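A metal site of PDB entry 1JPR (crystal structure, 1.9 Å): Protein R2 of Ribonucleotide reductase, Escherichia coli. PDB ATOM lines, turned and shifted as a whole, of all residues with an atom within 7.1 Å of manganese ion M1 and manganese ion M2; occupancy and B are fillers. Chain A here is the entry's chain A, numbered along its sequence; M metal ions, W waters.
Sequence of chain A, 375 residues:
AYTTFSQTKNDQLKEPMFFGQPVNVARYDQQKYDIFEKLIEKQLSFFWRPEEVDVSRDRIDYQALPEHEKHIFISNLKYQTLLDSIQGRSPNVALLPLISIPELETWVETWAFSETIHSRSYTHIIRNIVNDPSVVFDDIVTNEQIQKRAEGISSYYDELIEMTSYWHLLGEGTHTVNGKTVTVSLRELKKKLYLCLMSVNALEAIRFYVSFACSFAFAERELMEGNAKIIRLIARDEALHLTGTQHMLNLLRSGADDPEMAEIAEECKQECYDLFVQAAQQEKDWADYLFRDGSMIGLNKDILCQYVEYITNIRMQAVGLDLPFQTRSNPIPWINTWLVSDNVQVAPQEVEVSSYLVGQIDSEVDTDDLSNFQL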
ATOM      1  N   GLN A  80      29.259 -17.342  -6.325  1.00  0.00           N
ATOM      2  CA  GLN A  80      29.389 -18.487  -7.248  1.00  0.00           C
ATOM      3  C   GLN A  80      28.043 -19.264  -7.261  1.00  0.00           C
ATOM      4  O   GLN A  80      27.521 -19.664  -8.322  1.00  0.00           O
ATOM      5  CB  GLN A  80      30.526 -19.402  -6.799  1.00  0.00           C
ATOM      6  CG  GLN A  80      31.893 -18.675  -6.897  1.00  0.00           C
ATOM      7  CD  GLN A  80      33.081 -19.474  -6.295  1.00  0.00           C
ATOM      8  OE1 GLN A  80      32.936 -20.221  -5.301  1.00  0.00           O
ATOM      9  NE2 GLN A  80      34.256 -19.319  -6.905  1.00  0.00           N
ATOM     10  N   LEU A  83      25.456 -17.323  -9.278  1.00  0.00           N
ATOM     11  CA  LEU A  83      25.666 -17.407 -10.729  1.00  0.00           C
ATOM     12  C   LEU A  83      25.306 -18.766 -11.358  1.00  0.00           C
ATOM     13  O   LEU A  83      24.703 -18.833 -12.443  1.00  0.00           O
ATOM     14  CB  LEU A  83      27.135 -17.061 -11.063  1.00  0.00           C
ATOM     15  CG  LEU A  83      27.550 -15.574 -10.861  1.00  0.00           C
ATOM     16  CD1 LEU A  83      28.961 -15.384 -11.399  1.00  0.00           C
ATOM     17  CD2 LEU A  83      26.604 -14.651 -11.599  1.00  0.00           C
ATOM     18  N   ASP A  84      25.674 -19.856 -10.678  1.00  0.00           N
ATOM     19  CA  ASP A  84      25.424 -21.167 -11.255  1.00  0.00           C
ATOM     20  C   ASP A  84      23.952 -21.519 -11.081  1.00  0.00           C
ATOM     21  O   ASP A  84      23.449 -22.317 -11.870  1.00  0.00           O
ATOM     22  CB  ASP A  84      26.347 -22.241 -10.671  1.00  0.00           C
ATOM     23  CG  ASP A  84      27.721 -22.326 -11.415  1.00  0.00           C
ATOM     24  OD1 ASP A  84      27.727 -22.499 -12.619  1.00  0.00           O
ATOM     25  OD2 ASP A  84      28.795 -22.207 -10.836  1.00  0.00           O
ATOM     26  N   GLN A  87      22.743 -19.942 -14.177  1.00  0.00           N
ATOM     27  CA  GLN A  87      23.288 -20.599 -15.357  1.00  0.00           C
ATOM     28  C   GLN A  87      22.794 -22.017 -15.539  1.00  0.00           C
ATOM     29  O   GLN A  87      22.887 -22.560 -16.639  1.00  0.00           O
ATOM     30  CB  GLN A  87      24.845 -20.574 -15.318  1.00  0.00           C
ATOM     31  CG  GLN A  87      25.295 -19.105 -15.556  1.00  0.00           C
ATOM     32  CD  GLN A  87      24.959 -18.648 -16.949  1.00  0.00           C
ATOM     33  OE1 GLN A  87      25.612 -19.018 -17.923  1.00  0.00           O
ATOM     34  NE2 GLN A  87      23.915 -17.871 -17.070  1.00  0.00           N
ATOM     35  N   TRP A 111      25.743 -27.865 -21.509  1.00  0.00           N
ATOM     36  CA  TRP A 111      26.354 -26.752 -20.783  1.00  0.00           C
ATOM     37  C   TRP A 111      25.469 -26.459 -19.562  1.00  0.00           C
ATOM     38  O   TRP A 111      25.978 -26.384 -18.428  1.00  0.00           O
ATOM     39  CB  TRP A 111      26.364 -25.573 -21.750  1.00  0.00           C
ATOM     40  CG  TRP A 111      26.616 -24.185 -21.211  1.00  0.00           C
ATOM     41  CD1 TRP A 111      27.184 -23.831 -20.010  1.00  0.00           C
ATOM     42  CD2 TRP A 111      26.333 -22.979 -21.908  1.00  0.00           C
ATOM     43  NE1 TRP A 111      27.281 -22.418 -19.941  1.00  0.00           N
ATOM     44  CE2 TRP A 111      26.747 -21.890 -21.094  1.00  0.00           C
ATOM     45  CE3 TRP A 111      25.738 -22.684 -23.156  1.00  0.00           C
ATOM     46  CZ2 TRP A 111      26.577 -20.532 -21.508  1.00  0.00           C
ATOM     47  CZ3 TRP A 111      25.568 -21.349 -23.541  1.00  0.00           C
ATOM     48  CH2 TRP A 111      25.979 -20.292 -22.717  1.00  0.00           C
ATOM     49  N   SER A 114      25.804 -29.102 -16.942  1.00  0.00           N
ATOM     50  CA  SER A 114      27.068 -29.050 -16.214  1.00  0.00           C
ATOM     51  C   SER A 114      27.038 -27.976 -15.112  1.00  0.00           C
ATOM     52  O   SER A 114      27.731 -28.101 -14.110  1.00  0.00           O
ATOM     53  CB  SER A 114      28.254 -28.869 -17.203  1.00  0.00           C
ATOM     54  OG  SER A 114      28.281 -27.533 -17.677  1.00  0.00           O
ATOM     55  N   GLU A 115      26.230 -26.919 -15.296  1.00  0.00           N
ATOM     56  CA  GLU A 115      26.067 -25.871 -14.286  1.00  0.00           C
ATOM     57  C   GLU A 115      25.300 -26.442 -13.082  1.00  0.00           C
ATOM     58  O   GLU A 115      25.544 -26.051 -11.922  1.00  0.00           O
ATOM     59  CB  GLU A 115      25.307 -24.629 -14.876  1.00  0.00           C
ATOM     60  CG  GLU A 115      25.916 -23.996 -16.150  1.00  0.00           C
ATOM     61  CD  GLU A 115      27.306 -23.342 -15.919  1.00  0.00           C
ATOM     62  OE1 GLU A 115      28.031 -23.808 -15.023  1.00  0.00           O
ATOM     63  OE2 GLU A 115      27.680 -22.430 -16.658  1.00  0.00           O
ATOM     64  N   THR A 116      24.377 -27.349 -13.305  1.00  0.00           N
ATOM     65  CA  THR A 116      23.650 -27.926 -12.141  1.00  0.00           C
ATOM     66  C   THR A 116      24.593 -28.763 -11.312  1.00  0.00           C
ATOM     67  O   THR A 116      24.428 -28.870 -10.084  1.00  0.00           O
ATOM     68  CB  THR A 116      22.405 -28.818 -12.506  1.00  0.00           C
ATOM     69  OG1 THR A 116      22.827 -30.000 -13.207  1.00  0.00           O
ATOM     70  CG2 THR A 116      21.419 -28.006 -13.336  1.00  0.00           C
ATOM     71  N   HIS A 118      27.729 -27.931 -10.926  1.00  0.00           N
ATOM     72  CA  HIS A 118      28.446 -26.923 -10.102  1.00  0.00           C
ATOM     73  C   HIS A 118      27.616 -26.534  -8.889  1.00  0.00           C
ATOM     74  O   HIS A 118      28.121 -26.370  -7.732  1.00  0.00           O
ATOM     75  CB  HIS A 118      28.706 -25.704 -10.976  1.00  0.00           C
ATOM     76  CG  HIS A 118      29.575 -25.980 -12.147  1.00  0.00           C
ATOM     77  ND1 HIS A 118      29.904 -25.022 -13.046  1.00  0.00           N
ATOM     78  CD2 HIS A 118      30.225 -27.096 -12.545  1.00  0.00           C
ATOM     79  CE1 HIS A 118      30.723 -25.512 -13.951  1.00  0.00           C
ATOM     80  NE2 HIS A 118      30.935 -26.775 -13.665  1.00  0.00           N
ATOM     81  N   SER A 119      26.306 -26.325  -9.112  1.00  0.00           N
ATOM     82  CA  SER A 119      25.442 -25.964  -7.960  1.00  0.00           C
ATOM     83  C   SER A 119      25.450 -27.076  -6.912  1.00  0.00           C
ATOM     84  O   SER A 119      25.423 -26.828  -5.707  1.00  0.00           O
ATOM     85  CB  SER A 119      23.946 -25.754  -8.405  1.00  0.00           C
ATOM     86  OG  SER A 119      23.885 -24.686  -9.344  1.00  0.00           O
ATOM     87  N   TYR A 122      28.459 -26.809  -4.738  1.00  0.00           N
ATOM     88  CA  TYR A 122      28.421 -25.752  -3.677  1.00  0.00           C
ATOM     89  C   TYR A 122      27.614 -26.240  -2.462  1.00  0.00           C
ATOM     90  O   TYR A 122      27.947 -25.922  -1.283  1.00  0.00           O
ATOM     91  CB  TYR A 122      27.838 -24.459  -4.195  1.00  0.00           C
ATOM     92  CG  TYR A 122      28.514 -23.946  -5.431  1.00  0.00           C
ATOM     93  CD1 TYR A 122      29.905 -23.899  -5.532  1.00  0.00           C
ATOM     94  CD2 TYR A 122      27.758 -23.473  -6.506  1.00  0.00           C
ATOM     95  CE1 TYR A 122      30.541 -23.401  -6.689  1.00  0.00           C
ATOM     96  CE2 TYR A 122      28.363 -22.973  -7.653  1.00  0.00           C
ATOM     97  CZ  TYR A 122      29.749 -22.935  -7.744  1.00  0.00           C
ATOM     98  OH  TYR A 122      30.326 -22.400  -8.900  1.00  0.00           O
ATOM     99  N   VAL A 200      26.392 -13.175 -21.313  1.00  0.00           N
ATOM    100  CA  VAL A 200      26.760 -14.459 -20.766  1.00  0.00           C
ATOM    101  C   VAL A 200      28.250 -14.630 -20.961  1.00  0.00           C
ATOM    102  O   VAL A 200      28.950 -15.226 -20.108  1.00  0.00           O
ATOM    103  CB  VAL A 200      26.034 -15.609 -21.473  1.00  0.00           C
ATOM    104  CG1 VAL A 200      26.538 -16.933 -20.906  1.00  0.00           C
ATOM    105  CG2 VAL A 200      24.510 -15.465 -21.309  1.00  0.00           C
ATOM    106  N   LEU A 203      29.849 -12.967 -18.127  1.00  0.00           N
ATOM    107  CA  LEU A 203      29.604 -13.619 -16.892  1.00  0.00           C
ATOM    108  C   LEU A 203      30.601 -14.794 -16.709  1.00  0.00           C
ATOM    109  O   LEU A 203      31.231 -14.936 -15.668  1.00  0.00           O
ATOM    110  CB  LEU A 203      28.163 -14.167 -16.901  1.00  0.00           C
ATOM    111  CG  LEU A 203      27.624 -14.864 -15.638  1.00  0.00           C
ATOM    112  CD1 LEU A 203      26.092 -15.006 -15.810  1.00  0.00           C
ATOM    113  CD2 LEU A 203      28.258 -16.336 -15.493  1.00  0.00           C
ATOM    114  N   GLU A 204      30.745 -15.614 -17.725  1.00  0.00           N
ATOM    115  CA  GLU A 204      31.630 -16.771 -17.563  1.00  0.00           C
ATOM    116  C   GLU A 204      33.109 -16.477 -17.728  1.00  0.00           C
ATOM    117  O   GLU A 204      33.922 -17.087 -17.065  1.00  0.00           O
ATOM    118  CB  GLU A 204      31.190 -17.867 -18.517  1.00  0.00           C
ATOM    119  CG  GLU A 204      29.951 -18.531 -17.908  1.00  0.00           C
ATOM    120  CD  GLU A 204      29.346 -19.533 -18.811  1.00  0.00           C
ATOM    121  OE1 GLU A 204      28.792 -20.502 -18.294  1.00  0.00           O
ATOM    122  OE2 GLU A 204      29.420 -19.309 -20.027  1.00  0.00           O
ATOM    123  N   PHE A 208      33.120 -15.113 -13.300  1.00  0.00           N
ATOM    124  CA  PHE A 208      33.517 -16.358 -12.642  1.00  0.00           C
ATOM    125  C   PHE A 208      35.000 -16.427 -12.385  1.00  0.00           C
ATOM    126  O   PHE A 208      35.403 -17.024 -11.394  1.00  0.00           O
ATOM    127  CB  PHE A 208      33.078 -17.602 -13.430  1.00  0.00           C
ATOM    128  CG  PHE A 208      31.885 -18.286 -12.810  1.00  0.00           C
ATOM    129  CD1 PHE A 208      32.002 -18.839 -11.540  1.00  0.00           C
ATOM    130  CD2 PHE A 208      30.658 -18.281 -13.447  1.00  0.00           C
ATOM    131  CE1 PHE A 208      30.867 -19.397 -10.878  1.00  0.00           C
ATOM    132  CE2 PHE A 208      29.508 -18.820 -12.815  1.00  0.00           C
ATOM    133  CZ  PHE A 208      29.621 -19.383 -11.525  1.00  0.00           C
ATOM    134  N   PHE A 212      37.087 -17.197  -9.047  1.00  0.00           N
ATOM    135  CA  PHE A 212      38.067 -18.286  -8.923  1.00  0.00           C
ATOM    136  C   PHE A 212      39.321 -17.768  -8.235  1.00  0.00           C
ATOM    137  O   PHE A 212      39.890 -18.459  -7.405  1.00  0.00           O
ATOM    138  CB  PHE A 212      38.480 -18.846 -10.282  1.00  0.00           C
ATOM    139  CG  PHE A 212      37.369 -19.438 -11.060  1.00  0.00           C
ATOM    140  CD1 PHE A 212      36.281 -19.961 -10.437  1.00  0.00           C
ATOM    141  CD2 PHE A 212      37.448 -19.496 -12.481  1.00  0.00           C
ATOM    142  CE1 PHE A 212      35.219 -20.564 -11.216  1.00  0.00           C
ATOM    143  CE2 PHE A 212      36.403 -20.084 -13.239  1.00  0.00           C
ATOM    144  CZ  PHE A 212      35.306 -20.605 -12.586  1.00  0.00           C
ATOM    145  N   ILE A 234      35.433 -26.974 -11.682  1.00  0.00           N
ATOM    146  CA  ILE A 234      34.451 -25.985 -12.188  1.00  0.00           C
ATOM    147  C   ILE A 234      35.131 -25.072 -13.206  1.00  0.00           C
ATOM    148  O   ILE A 234      34.578 -24.832 -14.315  1.00  0.00           O
ATOM    149  CB  ILE A 234      33.871 -25.159 -11.045  1.00  0.00           C
ATOM    150  CG1 ILE A 234      32.900 -26.035 -10.238  1.00  0.00           C
ATOM    151  CG2 ILE A 234      33.175 -23.847 -11.613  1.00  0.00           C
ATOM    152  CD1 ILE A 234      32.373 -25.410  -8.968  1.00  0.00           C
ATOM    153  N   ASP A 237      35.437 -26.591 -16.595  1.00  0.00           N
ATOM    154  CA  ASP A 237      34.161 -26.572 -17.323  1.00  0.00           C
ATOM    155  C   ASP A 237      33.889 -25.146 -17.816  1.00  0.00           C
ATOM    156  O   ASP A 237      33.468 -24.953 -18.945  1.00  0.00           O
ATOM    157  CB  ASP A 237      32.971 -26.958 -16.417  1.00  0.00           C
ATOM    158  CG  ASP A 237      32.996 -28.371 -15.965  1.00  0.00           C
ATOM    159  OD1 ASP A 237      33.596 -29.228 -16.669  1.00  0.00           O
ATOM    160  OD2 ASP A 237      32.351 -28.643 -14.914  1.00  0.00           O
ATOM    161  N   GLU A 238      34.118 -24.127 -16.974  1.00  0.00           N
ATOM    162  CA  GLU A 238      33.872 -22.768 -17.439  1.00  0.00           C
ATOM    163  C   GLU A 238      34.719 -22.386 -18.656  1.00  0.00           C
ATOM    164  O   GLU A 238      34.249 -21.596 -19.514  1.00  0.00           O
ATOM    165  CB  GLU A 238      34.117 -21.741 -16.297  1.00  0.00           C
ATOM    166  CG  GLU A 238      33.003 -21.715 -15.222  1.00  0.00           C
ATOM    167  CD  GLU A 238      31.556 -21.809 -15.823  1.00  0.00           C
ATOM    168  OE1 GLU A 238      31.271 -21.045 -16.810  1.00  0.00           O
ATOM    169  OE2 GLU A 238      30.723 -22.642 -15.284  1.00  0.00           O
ATOM    170  N   ALA A 239      35.959 -22.919 -18.730  1.00  0.00           N
ATOM    171  CA  ALA A 239      36.819 -22.631 -19.909  1.00  0.00           C
ATOM    172  C   ALA A 239      36.087 -23.107 -21.183  1.00  0.00           C
ATOM    173  O   ALA A 239      36.134 -22.457 -22.230  1.00  0.00           O
ATOM    174  CB  ALA A 239      38.191 -23.337 -19.755  1.00  0.00           C
ATOM    175  N   HIS A 241      32.713 -23.417 -21.489  1.00  0.00           N
ATOM    176  CA  HIS A 241      31.498 -22.584 -21.630  1.00  0.00           C
ATOM    177  C   HIS A 241      31.819 -21.276 -22.312  1.00  0.00           C
ATOM    178  O   HIS A 241      31.094 -20.810 -23.207  1.00  0.00           O
ATOM    179  CB  HIS A 241      30.851 -22.324 -20.268  1.00  0.00           C
ATOM    180  CG  HIS A 241      30.496 -23.584 -19.565  1.00  0.00           C
ATOM    181  ND1 HIS A 241      30.033 -23.625 -18.269  1.00  0.00           N
ATOM    182  CD2 HIS A 241      30.566 -24.867 -19.981  1.00  0.00           C
ATOM    183  CE1 HIS A 241      29.828 -24.889 -17.915  1.00  0.00           C
ATOM    184  NE2 HIS A 241      30.145 -25.666 -18.949  1.00  0.00           N
ATOM    185  N   LEU A 242      32.924 -20.674 -21.904  1.00  0.00           N
ATOM    186  CA  LEU A 242      33.268 -19.389 -22.516  1.00  0.00           C
ATOM    187  C   LEU A 242      33.822 -19.584 -23.917  1.00  0.00           C
ATOM    188  O   LEU A 242      33.723 -18.676 -24.770  1.00  0.00           O
ATOM    189  CB  LEU A 242      34.196 -18.620 -21.605  1.00  0.00           C
ATOM    190  CG  LEU A 242      35.588 -19.159 -21.528  1.00  0.00           C
ATOM    191  CD1 LEU A 242      36.400 -18.489 -22.650  1.00  0.00           C
ATOM    192  CD2 LEU A 242      36.185 -18.789 -20.156  1.00  0.00           C
HETATM  193 MN    MN M   1      29.350 -23.028 -13.640  1.00  0.00          MN
HETATM  194 MN    MN M   2      29.593 -21.804 -16.845  1.00  0.00          MN
HETATM  195  O   HOH W   1      30.903 -21.698 -12.594  1.00  0.00           O
HETATM  196  O   HOH W   2      29.090 -20.200 -15.265  1.00  0.00           O
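The side-chain carboxylate (OD2) of Asp 84 is in hydrogen-bond range of the side-chain hydroxyl (OH) of Tyr 122. The backbone carbonyl oxygen (O) of Asp 84 is in hydrogen-bond range of the side-chain hydroxyl (OG) of Ser 119 (3.5 Å). The side-chain carboxylate (OE1) of Glu 204 sits close to the indole nitrogen (NE1) of Trp 111. The backbone carbonyl oxygen (O) of Ser 114 lies close to a ring nitrogen (NE2) of His 118, at 3.5 Å. OD2 of Asp 237 is in hydrogen-bond range of NE2 of His 118, 2.7 Å away. ND1 of His 241 lies close to NE1 of Trp 111 (3.4 Å). OG of Ser 114 sits at hydrogen-bond distance from NE2 of His 241, at 2.9 Å. O of Trp 111 lies within hydrogen-bond range of OG of Ser 114 (2.7 Å).
NE1 of Trp 111 touches manganese ion M2, 3.9 Å away. Five residues have an atom within 4 Å of manganese ion M2: Trp 111, Glu 115, Glu 204, Glu 238 and His 241.
Manganese ion M1 is bound by OD1 of Asp 84 (2.0 Å). OE1 of Glu 115 is bound to manganese ion M1 (2.1 Å). ND1 of His 118 binds manganese ion M1 (2.2 Å). Manganese ion M1 is bound by OE2 of Glu 238 (2.2 Å). Water W1 binds manganese ion M1, 2.3 Å away. Manganese ion M1 has five donor atoms within binding distance.
Manganese ion M2 is bound by OE1 of Glu 238, OE2 of Glu 115, OE2 of Glu 238, OE1 of Glu 204, water W2 and ND1 of His 241.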
